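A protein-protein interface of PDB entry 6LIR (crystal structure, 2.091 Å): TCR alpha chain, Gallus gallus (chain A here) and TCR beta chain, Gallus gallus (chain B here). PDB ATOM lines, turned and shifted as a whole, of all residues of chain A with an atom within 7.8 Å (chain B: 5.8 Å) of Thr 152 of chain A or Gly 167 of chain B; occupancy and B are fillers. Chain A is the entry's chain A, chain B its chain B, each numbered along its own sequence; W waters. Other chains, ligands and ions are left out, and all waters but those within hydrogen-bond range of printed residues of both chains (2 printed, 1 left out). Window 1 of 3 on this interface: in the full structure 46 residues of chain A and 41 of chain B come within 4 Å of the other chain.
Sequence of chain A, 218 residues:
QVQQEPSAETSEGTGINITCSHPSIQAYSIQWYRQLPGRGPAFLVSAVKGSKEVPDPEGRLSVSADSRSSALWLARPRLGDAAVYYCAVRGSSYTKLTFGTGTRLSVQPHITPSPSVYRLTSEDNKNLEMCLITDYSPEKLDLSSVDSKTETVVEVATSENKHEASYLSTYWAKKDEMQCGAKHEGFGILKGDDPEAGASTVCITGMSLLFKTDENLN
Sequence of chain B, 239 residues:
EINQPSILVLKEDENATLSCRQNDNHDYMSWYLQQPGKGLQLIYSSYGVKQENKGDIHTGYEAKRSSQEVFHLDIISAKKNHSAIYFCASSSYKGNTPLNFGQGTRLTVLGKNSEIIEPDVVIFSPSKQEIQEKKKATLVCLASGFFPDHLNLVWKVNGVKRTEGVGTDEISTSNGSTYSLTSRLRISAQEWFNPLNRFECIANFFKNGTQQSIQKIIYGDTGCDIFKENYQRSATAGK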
ATOM      1  N   LEU A  79      -1.895 -25.384 -13.997  1.00  0.00           N
ATOM      2  CA  LEU A  79      -0.717 -25.162 -14.831  1.00  0.00           C
ATOM      3  C   LEU A  79       0.523 -25.803 -14.222  1.00  0.00           C
ATOM      4  O   LEU A  79       1.370 -26.348 -14.941  1.00  0.00           O
ATOM      5  CB  LEU A  79      -0.505 -23.660 -15.031  1.00  0.00           C
ATOM      6  CG  LEU A  79       0.658 -23.213 -15.919  1.00  0.00           C
ATOM      7  CD1 LEU A  79       0.595 -23.894 -17.279  1.00  0.00           C
ATOM      8  CD2 LEU A  79       0.646 -21.699 -16.076  1.00  0.00           C
ATOM      9  N   ILE A 133       4.757 -12.122 -29.469  1.00  0.00           N
ATOM     10  CA  ILE A 133       3.310 -12.266 -29.591  1.00  0.00           C
ATOM     11  C   ILE A 133       2.751 -12.665 -28.231  1.00  0.00           C
ATOM     12  O   ILE A 133       3.174 -13.674 -27.654  1.00  0.00           O
ATOM     13  CB  ILE A 133       2.931 -13.295 -30.672  1.00  0.00           C
ATOM     14  CG1 ILE A 133       3.639 -12.977 -31.991  1.00  0.00           C
ATOM     15  CG2 ILE A 133       1.423 -13.319 -30.871  1.00  0.00           C
ATOM     16  CD1 ILE A 133       4.897 -13.799 -32.228  1.00  0.00           C
ATOM     17  N   TYR A 136      -2.624 -14.306 -26.666  1.00  0.00           N
ATOM     18  CA  TYR A 136      -3.355 -14.916 -27.766  1.00  0.00           C
ATOM     19  C   TYR A 136      -3.942 -16.252 -27.327  1.00  0.00           C
ATOM     20  O   TYR A 136      -3.668 -16.754 -26.232  1.00  0.00           O
ATOM     21  CB  TYR A 136      -2.440 -15.119 -28.979  1.00  0.00           C
ATOM     22  CG  TYR A 136      -1.227 -15.979 -28.684  1.00  0.00           C
ATOM     23  CD1 TYR A 136      -1.276 -17.362 -28.831  1.00  0.00           C
ATOM     24  CD2 TYR A 136      -0.037 -15.406 -28.255  1.00  0.00           C
ATOM     25  CE1 TYR A 136      -0.166 -18.150 -28.561  1.00  0.00           C
ATOM     26  CE2 TYR A 136       1.075 -16.184 -27.983  1.00  0.00           C
ATOM     27  CZ  TYR A 136       1.008 -17.554 -28.138  1.00  0.00           C
ATOM     28  OH  TYR A 136       2.116 -18.325 -27.866  1.00  0.00           O
ATOM     29  N   THR A 150       9.203 -20.080 -30.701  1.00  0.00           N
ATOM     30  CA  THR A 150       8.948 -20.904 -29.527  1.00  0.00           C
ATOM     31  C   THR A 150       7.828 -20.274 -28.711  1.00  0.00           C
ATOM     32  O   THR A 150       7.587 -19.068 -28.782  1.00  0.00           O
ATOM     33  CB  THR A 150      10.205 -21.078 -28.662  1.00  0.00           C
ATOM     34  OG1 THR A 150      10.905 -19.834 -28.568  1.00  0.00           O
ATOM     35  CG2 THR A 150      11.126 -22.132 -29.271  1.00  0.00           C
ATOM     36  N   GLU A 151       7.137 -21.106 -27.931  1.00  0.00           N
ATOM     37  CA  GLU A 151       5.928 -20.701 -27.226  1.00  0.00           C
ATOM     38  C   GLU A 151       6.021 -21.116 -25.766  1.00  0.00           C
ATOM     39  O   GLU A 151       6.621 -22.140 -25.437  1.00  0.00           O
ATOM     40  CB  GLU A 151       4.674 -21.324 -27.880  1.00  0.00           C
ATOM     41  CG  GLU A 151       3.406 -21.217 -27.053  1.00  0.00           C
ATOM     42  CD  GLU A 151       2.183 -21.766 -27.768  1.00  0.00           C
ATOM     43  OE1 GLU A 151       1.476 -20.975 -28.423  1.00  0.00           O
ATOM     44  OE2 GLU A 151       1.925 -22.985 -27.664  1.00  0.00           O
ATOM     45  N   THR A 152       5.421 -20.305 -24.892  1.00  0.00           N
ATOM     46  CA  THR A 152       5.356 -20.614 -23.472  1.00  0.00           C
ATOM     47  C   THR A 152       4.071 -20.034 -22.895  1.00  0.00           C
ATOM     48  O   THR A 152       3.348 -19.288 -23.557  1.00  0.00           O
ATOM     49  CB  THR A 152       6.560 -20.049 -22.711  1.00  0.00           C
ATOM     50  OG1 THR A 152       7.721 -20.096 -23.545  1.00  0.00           O
ATOM     51  CG2 THR A 152       6.814 -20.872 -21.470  1.00  0.00           C
ATOM     52  N   VAL A 153       3.793 -20.404 -21.643  1.00  0.00           N
ATOM     53  CA  VAL A 153       2.711 -19.837 -20.848  1.00  0.00           C
ATOM     54  C   VAL A 153       3.299 -19.407 -19.515  1.00  0.00           C
ATOM     55  O   VAL A 153       4.071 -20.150 -18.901  1.00  0.00           O
ATOM     56  CB  VAL A 153       1.557 -20.838 -20.615  1.00  0.00           C
ATOM     57  CG1 VAL A 153       0.270 -20.100 -20.281  1.00  0.00           C
ATOM     58  CG2 VAL A 153       1.371 -21.736 -21.811  1.00  0.00           C
ATOM     59  N   VAL A 154       2.930 -18.208 -19.063  1.00  0.00           N
ATOM     60  CA  VAL A 154       3.417 -17.677 -17.799  1.00  0.00           C
ATOM     61  C   VAL A 154       2.233 -17.128 -17.020  1.00  0.00           C
ATOM     62  O   VAL A 154       1.150 -16.898 -17.563  1.00  0.00           O
ATOM     63  CB  VAL A 154       4.485 -16.578 -17.990  1.00  0.00           C
ATOM     64  CG1 VAL A 154       5.674 -17.108 -18.778  1.00  0.00           C
ATOM     65  CG2 VAL A 154       3.879 -15.368 -18.683  1.00  0.00           C
ATOM     66  N   GLU A 155       2.456 -16.896 -15.732  1.00  0.00           N
ATOM     67  CA  GLU A 155       1.461 -16.281 -14.868  1.00  0.00           C
ATOM     68  C   GLU A 155       2.075 -15.032 -14.261  1.00  0.00           C
ATOM     69  O   GLU A 155       3.214 -15.069 -13.783  1.00  0.00           O
ATOM     70  CB  GLU A 155       1.006 -17.237 -13.762  1.00  0.00           C
ATOM     71  CG  GLU A 155       0.283 -18.478 -14.245  1.00  0.00           C
ATOM     72  CD  GLU A 155      -0.168 -19.362 -13.097  1.00  0.00           C
ATOM     73  OE1 GLU A 155      -1.377 -19.675 -13.024  1.00  0.00           O
ATOM     74  OE2 GLU A 155       0.685 -19.744 -12.269  1.00  0.00           O
ATOM     75  N   SER A 166      -1.069 -16.139 -19.429  1.00  0.00           N
ATOM     76  CA  SER A 166      -1.008 -15.593 -20.772  1.00  0.00           C
ATOM     77  C   SER A 166       0.030 -16.364 -21.567  1.00  0.00           C
ATOM     78  O   SER A 166       1.072 -16.751 -21.034  1.00  0.00           O
ATOM     79  CB  SER A 166      -0.656 -14.098 -20.759  1.00  0.00           C
ATOM     80  OG  SER A 166       0.584 -13.866 -20.108  1.00  0.00           O
ATOM     81  N   TYR A 167      -0.264 -16.575 -22.843  1.00  0.00           N
ATOM     82  CA  TYR A 167       0.659 -17.245 -23.739  1.00  0.00           C
ATOM     83  C   TYR A 167       1.614 -16.221 -24.329  1.00  0.00           C
ATOM     84  O   TYR A 167       1.265 -15.052 -24.515  1.00  0.00           O
ATOM     85  CB  TYR A 167      -0.094 -17.948 -24.871  1.00  0.00           C
ATOM     86  CG  TYR A 167      -0.665 -19.299 -24.515  1.00  0.00           C
ATOM     87  CD1 TYR A 167      -1.853 -19.409 -23.803  1.00  0.00           C
ATOM     88  CD2 TYR A 167      -0.020 -20.470 -24.904  1.00  0.00           C
ATOM     89  CE1 TYR A 167      -2.383 -20.649 -23.484  1.00  0.00           C
ATOM     90  CE2 TYR A 167      -0.541 -21.707 -24.594  1.00  0.00           C
ATOM     91  CZ  TYR A 167      -1.720 -21.793 -23.881  1.00  0.00           C
ATOM     92  OH  TYR A 167      -2.235 -23.029 -23.567  1.00  0.00           O
ATOM     93  N   LEU A 168       2.821 -16.681 -24.653  1.00  0.00           N
ATOM     94  CA  LEU A 168       3.828 -15.844 -25.286  1.00  0.00           C
ATOM     95  C   LEU A 168       4.546 -16.680 -26.328  1.00  0.00           C
ATOM     96  O   LEU A 168       4.918 -17.825 -26.061  1.00  0.00           O
ATOM     97  CB  LEU A 168       4.852 -15.310 -24.271  1.00  0.00           C
ATOM     98  CG  LEU A 168       4.378 -14.665 -22.970  1.00  0.00           C
ATOM     99  CD1 LEU A 168       5.553 -14.472 -22.015  1.00  0.00           C
ATOM    100  CD2 LEU A 168       3.688 -13.342 -23.250  1.00  0.00           C
ATOM    101  N   SER A 169       4.733 -16.104 -27.507  1.00  0.00           N
ATOM    102  CA  SER A 169       5.527 -16.701 -28.567  1.00  0.00           C
ATOM    103  C   SER A 169       6.588 -15.698 -28.987  1.00  0.00           C
ATOM    104  O   SER A 169       6.351 -14.489 -28.967  1.00  0.00           O
ATOM    105  CB  SER A 169       4.661 -17.115 -29.770  1.00  0.00           C
ATOM    106  OG  SER A 169       4.059 -18.384 -29.543  1.00  0.00           O
ATOM    107  N   THR A 170       7.766 -16.197 -29.358  1.00  0.00           N
ATOM    108  CA  THR A 170       8.838 -15.311 -29.788  1.00  0.00           C
ATOM    109  C   THR A 170       9.614 -15.938 -30.934  1.00  0.00           C
ATOM    110  O   THR A 170       9.695 -17.160 -31.060  1.00  0.00           O
ATOM    111  CB  THR A 170       9.836 -15.001 -28.655  1.00  0.00           C
ATOM    112  OG1 THR A 170      10.257 -16.223 -28.033  1.00  0.00           O
ATOM    113  CG2 THR A 170       9.220 -14.082 -27.614  1.00  0.00           C
ATOM    114  N   THR B 163      11.005 -17.575 -10.322  1.00  0.00           N
ATOM    115  CA  THR B 163      10.278 -18.515 -11.154  1.00  0.00           C
ATOM    116  C   THR B 163       8.921 -18.003 -11.606  1.00  0.00           C
ATOM    117  O   THR B 163       8.466 -18.360 -12.696  1.00  0.00           O
ATOM    118  CB  THR B 163      10.040 -19.824 -10.384  1.00  0.00           C
ATOM    119  OG1 THR B 163       9.590 -19.522  -9.055  1.00  0.00           O
ATOM    120  CG2 THR B 163      11.308 -20.649 -10.300  1.00  0.00           C
ATOM    121  N   GLY B 165       6.269 -16.034 -13.371  1.00  0.00           N
ATOM    122  CA  GLY B 165       6.246 -15.289 -14.602  1.00  0.00           C
ATOM    123  C   GLY B 165       7.324 -15.654 -15.590  1.00  0.00           C
ATOM    124  O   GLY B 165       7.432 -14.996 -16.632  1.00  0.00           O
ATOM    125  N   VAL B 166       8.104 -16.698 -15.326  1.00  0.00           N
ATOM    126  CA  VAL B 166       9.184 -17.097 -16.217  1.00  0.00           C
ATOM    127  C   VAL B 166       8.668 -18.184 -17.147  1.00  0.00           C
ATOM    128  O   VAL B 166       8.080 -19.178 -16.696  1.00  0.00           O
ATOM    129  CB  VAL B 166      10.406 -17.585 -15.422  1.00  0.00           C
ATOM    130  CG1 VAL B 166      11.469 -18.154 -16.358  1.00  0.00           C
ATOM    131  CG2 VAL B 166      10.979 -16.447 -14.592  1.00  0.00           C
ATOM    132  N   GLY B 167       8.865 -17.989 -18.448  1.00  0.00           N
ATOM    133  CA  GLY B 167       8.703 -19.082 -19.384  1.00  0.00           C
ATOM    134  C   GLY B 167       9.964 -19.340 -20.174  1.00  0.00           C
ATOM    135  O   GLY B 167      10.361 -18.511 -20.997  1.00  0.00           O
ATOM    136  N   THR B 168      10.577 -20.499 -19.969  1.00  0.00           N
ATOM    137  CA  THR B 168      11.825 -20.862 -20.625  1.00  0.00           C
ATOM    138  C   THR B 168      11.567 -21.993 -21.607  1.00  0.00           C
ATOM    139  O   THR B 168      10.882 -22.963 -21.264  1.00  0.00           O
ATOM    140  CB  THR B 168      12.882 -21.270 -19.596  1.00  0.00           C
ATOM    141  OG1 THR B 168      13.072 -20.196 -18.664  1.00  0.00           O
ATOM    142  CG2 THR B 168      14.202 -21.581 -20.279  1.00  0.00           C
ATOM    143  N   ASP B 169      12.092 -21.864 -22.826  1.00  0.00           N
ATOM    144  CA  ASP B 169      11.993 -22.962 -23.778  1.00  0.00           C
ATOM    145  C   ASP B 169      12.618 -24.215 -23.183  1.00  0.00           C
ATOM    146  O   ASP B 169      13.713 -24.170 -22.614  1.00  0.00           O
ATOM    147  CB  ASP B 169      12.697 -22.610 -25.090  1.00  0.00           C
ATOM    148  CG  ASP B 169      12.109 -21.394 -25.758  1.00  0.00           C
ATOM    149  OD1 ASP B 169      10.983 -21.004 -25.385  1.00  0.00           O
ATOM    150  OD2 ASP B 169      12.770 -20.830 -26.656  1.00  0.00           O
ATOM    151  N   THR B 182      15.555 -19.377 -25.588  1.00  0.00           N
ATOM    152  CA  THR B 182      14.860 -18.155 -25.215  1.00  0.00           C
ATOM    153  C   THR B 182      14.151 -18.337 -23.882  1.00  0.00           C
ATOM    154  O   THR B 182      13.561 -19.388 -23.619  1.00  0.00           O
ATOM    155  CB  THR B 182      13.841 -17.751 -26.298  1.00  0.00           C
ATOM    156  OG1 THR B 182      14.513 -17.594 -27.554  1.00  0.00           O
ATOM    157  CG2 THR B 182      13.148 -16.446 -25.940  1.00  0.00           C
ATOM    158  N   SER B 183      14.182 -17.293 -23.058  1.00  0.00           N
ATOM    159  CA  SER B 183      13.444 -17.276 -21.804  1.00  0.00           C
ATOM    160  C   SER B 183      12.775 -15.925 -21.650  1.00  0.00           C
ATOM    161  O   SER B 183      13.396 -14.886 -21.895  1.00  0.00           O
ATOM    162  CB  SER B 183      14.360 -17.540 -20.604  1.00  0.00           C
ATOM    163  OG  SER B 183      13.590 -17.644 -19.420  1.00  0.00           O
ATOM    164  N   ARG B 184      11.507 -15.947 -21.260  1.00  0.00           N
ATOM    165  CA  ARG B 184      10.720 -14.742 -21.061  1.00  0.00           C
ATOM    166  C   ARG B 184      10.343 -14.635 -19.594  1.00  0.00           C
ATOM    167  O   ARG B 184       9.896 -15.617 -18.993  1.00  0.00           O
ATOM    168  CB  ARG B 184       9.474 -14.748 -21.952  1.00  0.00           C
ATOM    169  CG  ARG B 184       9.800 -14.562 -23.426  1.00  0.00           C
ATOM    170  CD  ARG B 184       9.139 -15.620 -24.304  1.00  0.00           C
ATOM    171  NE  ARG B 184       9.518 -16.972 -23.920  1.00  0.00           N
ATOM    172  CZ  ARG B 184       9.807 -17.946 -24.778  1.00  0.00           C
ATOM    173  NH1 ARG B 184       9.777 -17.728 -26.085  1.00  0.00           N
ATOM    174  NH2 ARG B 184      10.135 -19.142 -24.321  1.00  0.00           N
ATOM    175  N   LEU B 185      10.563 -13.460 -19.014  1.00  0.00           N
ATOM    176  CA  LEU B 185      10.051 -13.115 -17.693  1.00  0.00           C
ATOM    177  C   LEU B 185       9.056 -11.975 -17.869  1.00  0.00           C
ATOM    178  O   LEU B 185       9.441 -10.863 -18.246  1.00  0.00           O
ATOM    179  CB  LEU B 185      11.183 -12.719 -16.745  1.00  0.00           C
ATOM    180  CG  LEU B 185      10.781 -11.989 -15.459  1.00  0.00           C
ATOM    181  CD1 LEU B 185       9.829 -12.833 -14.615  1.00  0.00           C
ATOM    182  CD2 LEU B 185      12.012 -11.584 -14.648  1.00  0.00           C
HETATM  183  O   HOH W   1       5.409 -20.544 -16.505  1.00  0.00           O
HETATM  184  O   HOH W   2       4.891 -18.226 -14.571  1.00  0.00           O
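The side-chain hydroxyl (OG1) of Thr 150 of chain A is in hydrogen-bond range of the side-chain carboxylate (OD2) of Asp 169 of chain B. O of Glu 155 of chain A lies close to N of Gly 165 of chain B (3.2 Å). The guanidinium group (NH1) of Arg 184 of chain B sits at hydrogen-bond distance from the side-chain hydroxyl (OG1) of Thr 150 of chain A (3.4 Å). OG1 of Thr 152 of chain A lies within hydrogen-bond range of NH2 of Arg 184 of chain B, 2.7 Å away. The side-chain hydroxyl (OG1) of Thr 170 of chain A lies within hydrogen-bond range of the guanidinium group (NH1) of Arg 184 of chain B.
The backbone carbonyl oxygen (O) of Thr 150 of chain A is in hydrogen-bond range of the backbone NH (N) of Thr 170 of chain A (2.9 Å). O of Leu 168 of chain A lies within hydrogen-bond range of N of Thr 152 of chain A. N of Gly 167 of chain B sits at hydrogen-bond distance from O of Arg 184 of chain B. OD1 of Asp 169 of chain B is in salt-bridge range of NH1 of Arg 184 of chain B. OH of Tyr 136 of chain A lies close to O of Leu 168 of chain A (3.4 Å). The backbone carbonyl oxygen (O) of Thr 182 of chain B sits at hydrogen-bond distance from the backbone NH (N) of Asp 169 of chain B (3.0 Å).
Among the printed residues, pairs that only touch across the chains: Thr 152 of chain A with Gly 167 of chain B (3.3 Å), Thr 152 of chain A with Asp 169 of chain B (3.9 Å), Val 154 of chain A with Gly 165 of chain B (3.5 Å), Val 154 of chain A with Val 166 of chain B (3.6 Å), Val 154 of chain A with Gly 167 of chain B (3.3 Å), Leu 168 of chain A with Arg 184 of chain B (3.9 Å) and Thr 170 of chain A with Thr 182 of chain B (3.6 Å).
Among the printed residues, no Asp or Glu carboxylate lies within 4 Å of a Lys or Arg side-chain nitrogen of the other chain.
Water W1 bridges the backbone carbonyl oxygen of Val 153 of chain A (2.8 Å) and the backbone carbonyl oxygen of Val 166 of chain B (3.0 Å). Water W2 bridges N of Gly 165 of chain B and N of Glu 155 of chain A.
Of chain B, only Gly 167 (3.3 Å), Asp 169 (3.9 Å) and Arg 184 (2.7 Å) come within 4 Å of Thr 152 of chain A. Of chain A, only Thr 152 (3.3 Å) and Val 154 (3.3 Å) come within 4 Å of Gly 167 of chain B. Printed residues of chain A within 4 Å of Gly 165 of chain B: Val 154 (3.5 Å) and Glu 155 (3.1 Å). Of the printed residues of chain B, Glu 155 of chain A touches Gly 165 (3.1 Å). Of the printed residues of chain B, Thr 150 of chain A touches Asp 169 (2.9 Å) and Arg 184 (3.4 Å). Leu 79 of chain A touches none of the printed residues of chain B. The nearest residue of chain B that does not touch Thr 152 of chain A is Thr 168 of chain B (4.1 Å). The nearest residue of chain A that does not touch Gly 167 of chain B is Val 153 of chain A (4.8 Å).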
